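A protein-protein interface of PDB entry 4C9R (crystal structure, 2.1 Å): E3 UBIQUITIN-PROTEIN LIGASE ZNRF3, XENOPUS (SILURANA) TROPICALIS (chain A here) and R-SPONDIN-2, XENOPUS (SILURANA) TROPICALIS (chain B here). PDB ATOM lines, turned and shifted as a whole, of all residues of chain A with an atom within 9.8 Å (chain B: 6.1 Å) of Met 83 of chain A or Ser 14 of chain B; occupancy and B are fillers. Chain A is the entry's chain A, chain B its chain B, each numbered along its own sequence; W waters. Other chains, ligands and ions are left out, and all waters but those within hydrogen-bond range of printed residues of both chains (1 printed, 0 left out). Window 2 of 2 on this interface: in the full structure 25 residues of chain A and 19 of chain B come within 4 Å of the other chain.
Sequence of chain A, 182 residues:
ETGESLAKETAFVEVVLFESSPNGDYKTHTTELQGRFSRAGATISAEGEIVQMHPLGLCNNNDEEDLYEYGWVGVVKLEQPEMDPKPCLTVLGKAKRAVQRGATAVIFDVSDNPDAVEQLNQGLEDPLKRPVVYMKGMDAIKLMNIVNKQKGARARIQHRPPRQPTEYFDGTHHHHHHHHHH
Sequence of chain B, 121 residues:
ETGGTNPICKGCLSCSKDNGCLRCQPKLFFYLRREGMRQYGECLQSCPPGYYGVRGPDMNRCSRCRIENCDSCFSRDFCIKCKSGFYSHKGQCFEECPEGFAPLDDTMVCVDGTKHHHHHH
Water W1 bridges the side-chain carboxylate of Asp 84 of chain A and the guanidinium group of Arg 23 of chain B.
Leu 22 of chain B touches His 54 of chain A (CD2 to CE1, 3.7 Å).
Leu 22 of chain B touches Leu 56 of chain A (O to CD1, 3.2 Å).
Glu 79 of chain A touches Leu 22 of chain B.
O of Met 83 of chain A touches CD of Arg 23 of chain B, 3.5 Å away.
CD of Pro 85 of chain A touches NH1 of Arg 23 of chain B, 3.5 Å away.
N of Leu 56 of chain A sits at hydrogen-bond distance from ND1 of His 54 of chain A (3.2 Å).
SG of Cys 21 of chain B is disulfide-bonded to SG of Cys 12 of chain B, 2.1 Å away.
The backbone carbonyl oxygen (O) of Arg 23 of chain B lies within hydrogen-bond range of the backbone NH (N) of Leu 13 of chain B.
The backbone NH (N) of Leu 22 of chain B sits at hydrogen-bond distance from the backbone carbonyl oxygen (O) of Ser 14 of chain B, 2.8 Å away.
The backbone NH (N) of Ser 14 of chain B lies within hydrogen-bond range of the backbone carbonyl oxygen (O) of Arg 23 of chain B, 3.4 Å away.
Of the printed residues of chain B, His 54 of chain A touches Cys 21 (3.0 Å) and Leu 22 (3.7 Å).
Of the printed residues of chain B, Leu 56 of chain A touches Leu 22 (3.2 Å).
Met 83 of chain A touches two residues of chain B.
No residue of chain A comes within 4 Å of Cys 12 of chain B.
No residue of chain A comes within 4 Å of Leu 13 of chain B.
No residue of chain A comes within 4 Å of Cys 15 of chain B.
Of the printed residues of chain A, Ser 16 of chain B touches Glu 79.
Cys 21 of chain B touches just one residue of chain A: His 54.
Of chain A, only His 54 (3.7 Å), Leu 56 (3.2 Å) and Glu 79 (3.6 Å) come within 4 Å of Leu 22 of chain B.
Printed residues of chain A within 4 Å of Arg 23 of chain B: Met 83 (3.5 Å) and Pro 85 (3.5 Å).
The nearest residue of chain B that does not touch Met 83 of chain A is Leu 22 of chain B (4.3 Å).
Of the 17 printed residues of chain A, 5 touch a printed residue of chain B.
Printed residues of chain A that touch a printed residue of chain B: His 54, Leu 56, Glu 79, Met 83 and Pro 85.
Along chain A the printed residues that touch a printed residue of chain B span positions 54 to 85.
Printed residues of chain B that touch a printed residue of chain A: Ser 14, Ser 16, Cys 21, Leu 22 and Arg 23.
NE2 of His 54 of chain A lies within hydrogen-bond range of O of Cys 21 of chain B, 3.0 Å away.
The side-chain carboxylate (OE2) of Glu 79 of chain A is in hydrogen-bond range of the side-chain hydroxyl (OG) of Ser 16 of chain B (2.7 Å).
The side-chain sulfur (SD) of Met 83 of chain A sits at hydrogen-bond distance from the side-chain hydroxyl (OG) of Ser 14 of chain B.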
ATOM      1  N   HIS A  54      16.124 -31.351 -19.288  1.00  0.00           N
ATOM      2  CA  HIS A  54      17.270 -30.866 -18.502  1.00  0.00           C
ATOM      3  C   HIS A  54      18.318 -30.398 -19.528  1.00  0.00           C
ATOM      4  O   HIS A  54      18.603 -31.127 -20.479  1.00  0.00           O
ATOM      5  CB  HIS A  54      17.794 -32.013 -17.666  1.00  0.00           C
ATOM      6  CG  HIS A  54      18.744 -31.611 -16.585  1.00  0.00           C
ATOM      7  ND1 HIS A  54      19.959 -31.017 -16.841  1.00  0.00           N
ATOM      8  CD2 HIS A  54      18.667 -31.742 -15.236  1.00  0.00           C
ATOM      9  CE1 HIS A  54      20.568 -30.750 -15.700  1.00  0.00           C
ATOM     10  NE2 HIS A  54      19.825 -31.217 -14.716  1.00  0.00           N
ATOM     11  N   PRO A  55      18.904 -29.212 -19.345  1.00  0.00           N
ATOM     12  CA  PRO A  55      19.865 -28.728 -20.354  1.00  0.00           C
ATOM     13  C   PRO A  55      21.033 -29.692 -20.584  1.00  0.00           C
ATOM     14  O   PRO A  55      21.474 -29.852 -21.707  1.00  0.00           O
ATOM     15  CB  PRO A  55      20.384 -27.408 -19.772  1.00  0.00           C
ATOM     16  CG  PRO A  55      19.846 -27.302 -18.413  1.00  0.00           C
ATOM     17  CD  PRO A  55      18.681 -28.220 -18.284  1.00  0.00           C
ATOM     18  N   LEU A  56      21.518 -30.319 -19.524  1.00  0.00           N
ATOM     19  CA  LEU A  56      22.678 -31.209 -19.624  1.00  0.00           C
ATOM     20  C   LEU A  56      22.422 -32.516 -20.327  1.00  0.00           C
ATOM     21  O   LEU A  56      23.344 -33.195 -20.698  1.00  0.00           O
ATOM     22  CB  LEU A  56      23.161 -31.578 -18.256  1.00  0.00           C
ATOM     23  CG  LEU A  56      23.908 -30.474 -17.546  1.00  0.00           C
ATOM     24  CD1 LEU A  56      24.073 -30.864 -16.081  1.00  0.00           C
ATOM     25  CD2 LEU A  56      25.258 -30.352 -18.214  1.00  0.00           C
ATOM     26  N   LYS A  77      14.973 -25.008 -19.169  1.00  0.00           N
ATOM     27  CA  LYS A  77      15.327 -24.011 -18.229  1.00  0.00           C
ATOM     28  C   LYS A  77      16.859 -23.942 -18.143  1.00  0.00           C
ATOM     29  O   LYS A  77      17.520 -24.845 -17.645  1.00  0.00           O
ATOM     30  CB  LYS A  77      14.661 -24.334 -16.893  1.00  0.00           C
ATOM     31  CG  LYS A  77      15.189 -23.553 -15.711  1.00  0.00           C
ATOM     32  CD  LYS A  77      14.634 -22.179 -15.653  1.00  0.00           C
ATOM     33  CE  LYS A  77      15.230 -21.378 -14.475  1.00  0.00           C
ATOM     34  NZ  LYS A  77      14.800 -19.957 -14.643  1.00  0.00           N
ATOM     35  N   LEU A  78      17.393 -22.843 -18.628  1.00  0.00           N
ATOM     36  CA  LEU A  78      18.814 -22.589 -18.612  1.00  0.00           C
ATOM     37  C   LEU A  78      19.298 -22.114 -17.241  1.00  0.00           C
ATOM     38  O   LEU A  78      18.610 -21.372 -16.500  1.00  0.00           O
ATOM     39  CB  LEU A  78      19.181 -21.551 -19.676  1.00  0.00           C
ATOM     40  CG  LEU A  78      18.984 -21.924 -21.154  1.00  0.00           C
ATOM     41  CD1 LEU A  78      19.358 -20.723 -21.987  1.00  0.00           C
ATOM     42  CD2 LEU A  78      19.754 -23.174 -21.630  1.00  0.00           C
ATOM     43  N   GLU A  79      20.473 -22.586 -16.873  1.00  0.00           N
ATOM     44  CA  GLU A  79      21.062 -22.218 -15.584  1.00  0.00           C
ATOM     45  C   GLU A  79      22.143 -21.148 -15.780  1.00  0.00           C
ATOM     46  O   GLU A  79      22.494 -20.760 -16.908  1.00  0.00           O
ATOM     47  CB  GLU A  79      21.628 -23.448 -14.879  1.00  0.00           C
ATOM     48  CG  GLU A  79      20.600 -24.547 -14.640  1.00  0.00           C
ATOM     49  CD  GLU A  79      19.523 -24.209 -13.610  1.00  0.00           C
ATOM     50  OE1 GLU A  79      19.745 -23.288 -12.817  1.00  0.00           O
ATOM     51  OE2 GLU A  79      18.468 -24.875 -13.575  1.00  0.00           O
ATOM     52  N   GLN A  80      22.681 -20.698 -14.665  1.00  0.00           N
ATOM     53  CA  GLN A  80      23.735 -19.670 -14.642  1.00  0.00           C
ATOM     54  C   GLN A  80      24.894 -20.260 -15.464  1.00  0.00           C
ATOM     55  O   GLN A  80      25.234 -21.427 -15.299  1.00  0.00           O
ATOM     56  CB  GLN A  80      24.105 -19.384 -13.166  1.00  0.00           C
ATOM     57  CG  GLN A  80      24.404 -17.957 -12.739  1.00  0.00           C
ATOM     58  CD  GLN A  80      23.324 -16.925 -13.064  1.00  0.00           C
ATOM     59  OE1 GLN A  80      22.257 -16.881 -12.442  1.00  0.00           O
ATOM     60  NE2 GLN A  80      23.622 -16.055 -14.024  1.00  0.00           N
ATOM     61  N   PRO A  81      25.471 -19.484 -16.391  1.00  0.00           N
ATOM     62  CA  PRO A  81      26.510 -20.033 -17.266  1.00  0.00           C
ATOM     63  C   PRO A  81      27.590 -20.898 -16.568  1.00  0.00           C
ATOM     64  O   PRO A  81      28.034 -21.913 -17.132  1.00  0.00           O
ATOM     65  CB  PRO A  81      27.155 -18.775 -17.880  1.00  0.00           C
ATOM     66  CG  PRO A  81      26.144 -17.674 -17.737  1.00  0.00           C
ATOM     67  CD  PRO A  81      25.338 -18.015 -16.524  1.00  0.00           C
ATOM     68  N   GLU A  82      27.999 -20.526 -15.355  1.00  0.00           N
ATOM     69  CA  GLU A  82      29.147 -21.183 -14.721  1.00  0.00           C
ATOM     70  C   GLU A  82      28.813 -22.563 -14.194  1.00  0.00           C
ATOM     71  O   GLU A  82      29.701 -23.317 -13.812  1.00  0.00           O
ATOM     72  CB  GLU A  82      29.773 -20.330 -13.602  1.00  0.00           C
ATOM     73  CG  GLU A  82      28.943 -20.162 -12.340  1.00  0.00           C
ATOM     74  CD  GLU A  82      27.886 -19.056 -12.441  1.00  0.00           C
ATOM     75  OE1 GLU A  82      27.744 -18.399 -13.508  1.00  0.00           O
ATOM     76  OE2 GLU A  82      27.163 -18.855 -11.440  1.00  0.00           O
ATOM     77  N   MET A  83      27.539 -22.903 -14.193  1.00  0.00           N
ATOM     78  CA  MET A  83      27.128 -24.241 -13.771  1.00  0.00           C
ATOM     79  C   MET A  83      27.468 -25.306 -14.802  1.00  0.00           C
ATOM     80  O   MET A  83      27.424 -26.484 -14.475  1.00  0.00           O
ATOM     81  CB  MET A  83      25.628 -24.296 -13.541  1.00  0.00           C
ATOM     82  CG  MET A  83      25.055 -23.153 -12.724  1.00  0.00           C
ATOM     83  SD  MET A  83      25.409 -23.385 -10.992  1.00  0.00           S
ATOM     84  CE  MET A  83      23.945 -22.609 -10.317  1.00  0.00           C
ATOM     85  N   ASP A  84      27.779 -24.909 -16.042  1.00  0.00           N
ATOM     86  CA  ASP A  84      28.095 -25.884 -17.109  1.00  0.00           C
ATOM     87  C   ASP A  84      29.320 -25.377 -17.841  1.00  0.00           C
ATOM     88  O   ASP A  84      29.226 -24.809 -18.925  1.00  0.00           O
ATOM     89  CB  ASP A  84      26.910 -26.042 -18.077  1.00  0.00           C
ATOM     90  CG  ASP A  84      27.105 -27.182 -19.069  1.00  0.00           C
ATOM     91  OD1 ASP A  84      27.900 -28.106 -18.797  1.00  0.00           O
ATOM     92  OD2 ASP A  84      26.438 -27.173 -20.110  1.00  0.00           O
ATOM     93  N   PRO A  85      30.471 -25.529 -17.216  1.00  0.00           N
ATOM     94  CA  PRO A  85      31.664 -24.795 -17.638  1.00  0.00           C
ATOM     95  C   PRO A  85      32.248 -25.160 -19.023  1.00  0.00           C
ATOM     96  O   PRO A  85      32.913 -24.338 -19.680  1.00  0.00           O
ATOM     97  CB  PRO A  85      32.664 -25.102 -16.509  1.00  0.00           C
ATOM     98  CG  PRO A  85      32.146 -26.332 -15.832  1.00  0.00           C
ATOM     99  CD  PRO A  85      30.661 -26.234 -15.937  1.00  0.00           C
ATOM    100  N   LYS A  86      31.998 -26.376 -19.481  1.00  0.00           N
ATOM    101  CA  LYS A  86      32.324 -26.727 -20.857  1.00  0.00           C
ATOM    102  C   LYS A  86      31.131 -27.494 -21.441  1.00  0.00           C
ATOM    103  O   LYS A  86      31.076 -28.703 -21.380  1.00  0.00           O
ATOM    104  CB  LYS A  86      33.638 -27.516 -20.924  1.00  0.00           C
ATOM    105  CG  LYS A  86      34.568 -27.060 -22.063  1.00  0.00           C
ATOM    106  CD  LYS A  86      34.670 -28.047 -23.217  1.00  0.00           C
ATOM    107  CE  LYS A  86      33.398 -28.106 -24.054  1.00  0.00           C
ATOM    108  NZ  LYS A  86      33.326 -29.375 -24.851  1.00  0.00           N
ATOM    109  N   PRO A  87      30.147 -26.760 -21.959  1.00  0.00           N
ATOM    110  CA  PRO A  87      28.938 -27.348 -22.516  1.00  0.00           C
ATOM    111  C   PRO A  87      29.258 -28.389 -23.590  1.00  0.00           C
ATOM    112  O   PRO A  87      30.154 -28.150 -24.399  1.00  0.00           O
ATOM    113  CB  PRO A  87      28.243 -26.154 -23.179  1.00  0.00           C
ATOM    114  CG  PRO A  87      28.737 -24.958 -22.463  1.00  0.00           C
ATOM    115  CD  PRO A  87      30.143 -25.284 -22.038  1.00  0.00           C
ATOM    116  N   CYS A  88      28.525 -29.505 -23.582  1.00  0.00           N
ATOM    117  CA  CYS A  88      28.562 -30.507 -24.663  1.00  0.00           C
ATOM    118  C   CYS A  88      28.130 -29.892 -25.997  1.00  0.00           C
ATOM    119  O   CYS A  88      28.637 -30.266 -27.028  1.00  0.00           O
ATOM    120  CB  CYS A  88      27.686 -31.727 -24.314  1.00  0.00           C
ATOM    121  SG  CYS A  88      25.894 -31.399 -24.101  1.00  0.00           S
ATOM    122  N   ASP A 112      17.905 -16.962 -16.020  1.00  0.00           N
ATOM    123  CA  ASP A 112      19.264 -17.116 -15.442  1.00  0.00           C
ATOM    124  C   ASP A 112      20.474 -17.067 -16.381  1.00  0.00           C
ATOM    125  O   ASP A 112      21.606 -17.212 -15.952  1.00  0.00           O
ATOM    126  CB  ASP A 112      19.335 -18.437 -14.720  1.00  0.00           C
ATOM    127  CG  ASP A 112      18.415 -18.482 -13.511  1.00  0.00           C
ATOM    128  OD1 ASP A 112      17.927 -17.412 -13.063  1.00  0.00           O
ATOM    129  OD2 ASP A 112      18.172 -19.595 -13.010  1.00  0.00           O
ATOM    130  N   ASN A 113      20.240 -16.849 -17.658  1.00  0.00           N
ATOM    131  CA  ASN A 113      21.299 -16.823 -18.614  1.00  0.00           C
ATOM    132  C   ASN A 113      20.907 -15.878 -19.740  1.00  0.00           C
ATOM    133  O   ASN A 113      20.793 -16.268 -20.882  1.00  0.00           O
ATOM    134  CB  ASN A 113      21.555 -18.232 -19.114  1.00  0.00           C
ATOM    135  CG  ASN A 113      22.769 -18.326 -20.029  1.00  0.00           C
ATOM    136  OD1 ASN A 113      23.479 -17.363 -20.275  1.00  0.00           O
ATOM    137  ND2 ASN A 113      23.004 -19.509 -20.528  1.00  0.00           N
ATOM    138  N   CYS B  12      24.283 -33.516  -4.846  1.00  0.00           N
ATOM    139  CA  CYS B  12      24.788 -32.484  -5.764  1.00  0.00           C
ATOM    140  C   CYS B  12      25.535 -31.387  -5.089  1.00  0.00           C
ATOM    141  O   CYS B  12      25.221 -30.979  -3.967  1.00  0.00           O
ATOM    142  CB  CYS B  12      23.750 -31.842  -6.706  1.00  0.00           C
ATOM    143  SG  CYS B  12      22.018 -31.948  -6.306  1.00  0.00           S
ATOM    144  N   LEU B  13      26.538 -30.918  -5.813  1.00  0.00           N
ATOM    145  CA  LEU B  13      27.245 -29.731  -5.426  1.00  0.00           C
ATOM    146  C   LEU B  13      26.364 -28.545  -5.797  1.00  0.00           C
ATOM    147  O   LEU B  13      26.138 -27.678  -4.954  1.00  0.00           O
ATOM    148  CB  LEU B  13      28.615 -29.672  -6.090  1.00  0.00           C
ATOM    149  CG  LEU B  13      29.611 -30.590  -5.361  1.00  0.00           C
ATOM    150  CD1 LEU B  13      30.878 -30.750  -6.180  1.00  0.00           C
ATOM    151  CD2 LEU B  13      29.923 -30.087  -3.962  1.00  0.00           C
ATOM    152  N   SER B  14      25.828 -28.502  -7.020  1.00  0.00           N
ATOM    153  CA  SER B  14      24.814 -27.480  -7.297  1.00  0.00           C
ATOM    154  C   SER B  14      23.494 -28.077  -7.784  1.00  0.00           C
ATOM    155  O   SER B  14      23.457 -29.064  -8.518  1.00  0.00           O
ATOM    156  CB  SER B  14      25.343 -26.368  -8.199  1.00  0.00           C
ATOM    157  OG  SER B  14      25.682 -26.841  -9.480  1.00  0.00           O
ATOM    158  N   CYS B  15      22.415 -27.462  -7.315  1.00  0.00           N
ATOM    159  CA  CYS B  15      21.074 -27.958  -7.498  1.00  0.00           C
ATOM    160  C   CYS B  15      20.122 -26.842  -7.934  1.00  0.00           C
ATOM    161  O   CYS B  15      20.302 -25.680  -7.617  1.00  0.00           O
ATOM    162  CB  CYS B  15      20.567 -28.526  -6.204  1.00  0.00           C
ATOM    163  SG  CYS B  15      19.124 -29.580  -6.467  1.00  0.00           S
ATOM    164  N   SER B  16      19.073 -27.213  -8.624  1.00  0.00           N
ATOM    165  CA  SER B  16      18.132 -26.218  -9.099  1.00  0.00           C
ATOM    166  C   SER B  16      16.759 -26.744  -8.834  1.00  0.00           C
ATOM    167  O   SER B  16      16.486 -27.907  -8.979  1.00  0.00           O
ATOM    168  CB  SER B  16      18.372 -25.955 -10.585  1.00  0.00           C
ATOM    169  OG  SER B  16      17.198 -25.579 -11.241  1.00  0.00           O
ATOM    170  N   GLY B  20      16.661 -30.021 -10.780  1.00  0.00           N
ATOM    171  CA  GLY B  20      17.321 -30.925  -9.842  1.00  0.00           C
ATOM    172  C   GLY B  20      18.798 -30.656  -9.833  1.00  0.00           C
ATOM    173  O   GLY B  20      19.210 -29.539 -10.055  1.00  0.00           O
ATOM    174  N   CYS B  21      19.605 -31.686  -9.649  1.00  0.00           N
ATOM    175  CA  CYS B  21      21.058 -31.525  -9.665  1.00  0.00           C
ATOM    176  C   CYS B  21      21.602 -31.074 -11.012  1.00  0.00           C
ATOM    177  O   CYS B  21      21.156 -31.515 -12.064  1.00  0.00           O
ATOM    178  CB  CYS B  21      21.769 -32.827  -9.257  1.00  0.00           C
ATOM    179  SG  CYS B  21      21.346 -33.417  -7.575  1.00  0.00           S
ATOM    180  N   LEU B  22      22.597 -30.203 -10.950  1.00  0.00           N
ATOM    181  CA  LEU B  22      23.326 -29.731 -12.098  1.00  0.00           C
ATOM    182  C   LEU B  22      24.771 -30.252 -12.113  1.00  0.00           C
ATOM    183  O   LEU B  22      25.293 -30.540 -13.169  1.00  0.00           O
ATOM    184  CB  LEU B  22      23.315 -28.213 -12.110  1.00  0.00           C
ATOM    185  CG  LEU B  22      21.899 -27.642 -12.049  1.00  0.00           C
ATOM    186  CD1 LEU B  22      21.943 -26.163 -11.672  1.00  0.00           C
ATOM    187  CD2 LEU B  22      21.233 -27.890 -13.400  1.00  0.00           C
ATOM    188  N   ARG B  23      25.396 -30.357 -10.945  1.00  0.00           N
ATOM    189  CA  ARG B  23      26.655 -31.088 -10.776  1.00  0.00           C
ATOM    190  C   ARG B  23      26.618 -31.935  -9.515  1.00  0.00           C
ATOM    191  O   ARG B  23      26.125 -31.524  -8.453  1.00  0.00           O
ATOM    192  CB  ARG B  23      27.861 -30.146 -10.746  1.00  0.00           C
ATOM    193  CG  ARG B  23      28.134 -29.489 -12.096  1.00  0.00           C
ATOM    194  CD  ARG B  23      29.111 -28.312 -12.017  1.00  0.00           C
ATOM    195  NE  ARG B  23      30.518 -28.731 -12.010  1.00  0.00           N
ATOM    196  CZ  ARG B  23      31.187 -29.206 -13.066  1.00  0.00           C
ATOM    197  NH1 ARG B  23      30.594 -29.351 -14.255  1.00  0.00           N
ATOM    198  NH2 ARG B  23      32.465 -29.550 -12.933  1.00  0.00           N
ATOM    199  N   CYS B  24      27.136 -33.136  -9.663  1.00  0.00           N
ATOM    200  CA  CYS B  24      27.229 -34.097  -8.601  1.00  0.00           C
ATOM    201  C   CYS B  24      28.558 -33.922  -7.863  1.00  0.00           C
ATOM    202  O   CYS B  24      29.564 -33.561  -8.457  1.00  0.00           O
ATOM    203  CB  CYS B  24      27.151 -35.516  -9.197  1.00  0.00           C
ATOM    204  SG  CYS B  24      25.534 -35.913  -9.944  1.00  0.00           S
HETATM  205  O   HOH W   1      28.266 -30.168 -16.493  1.00  0.00           O
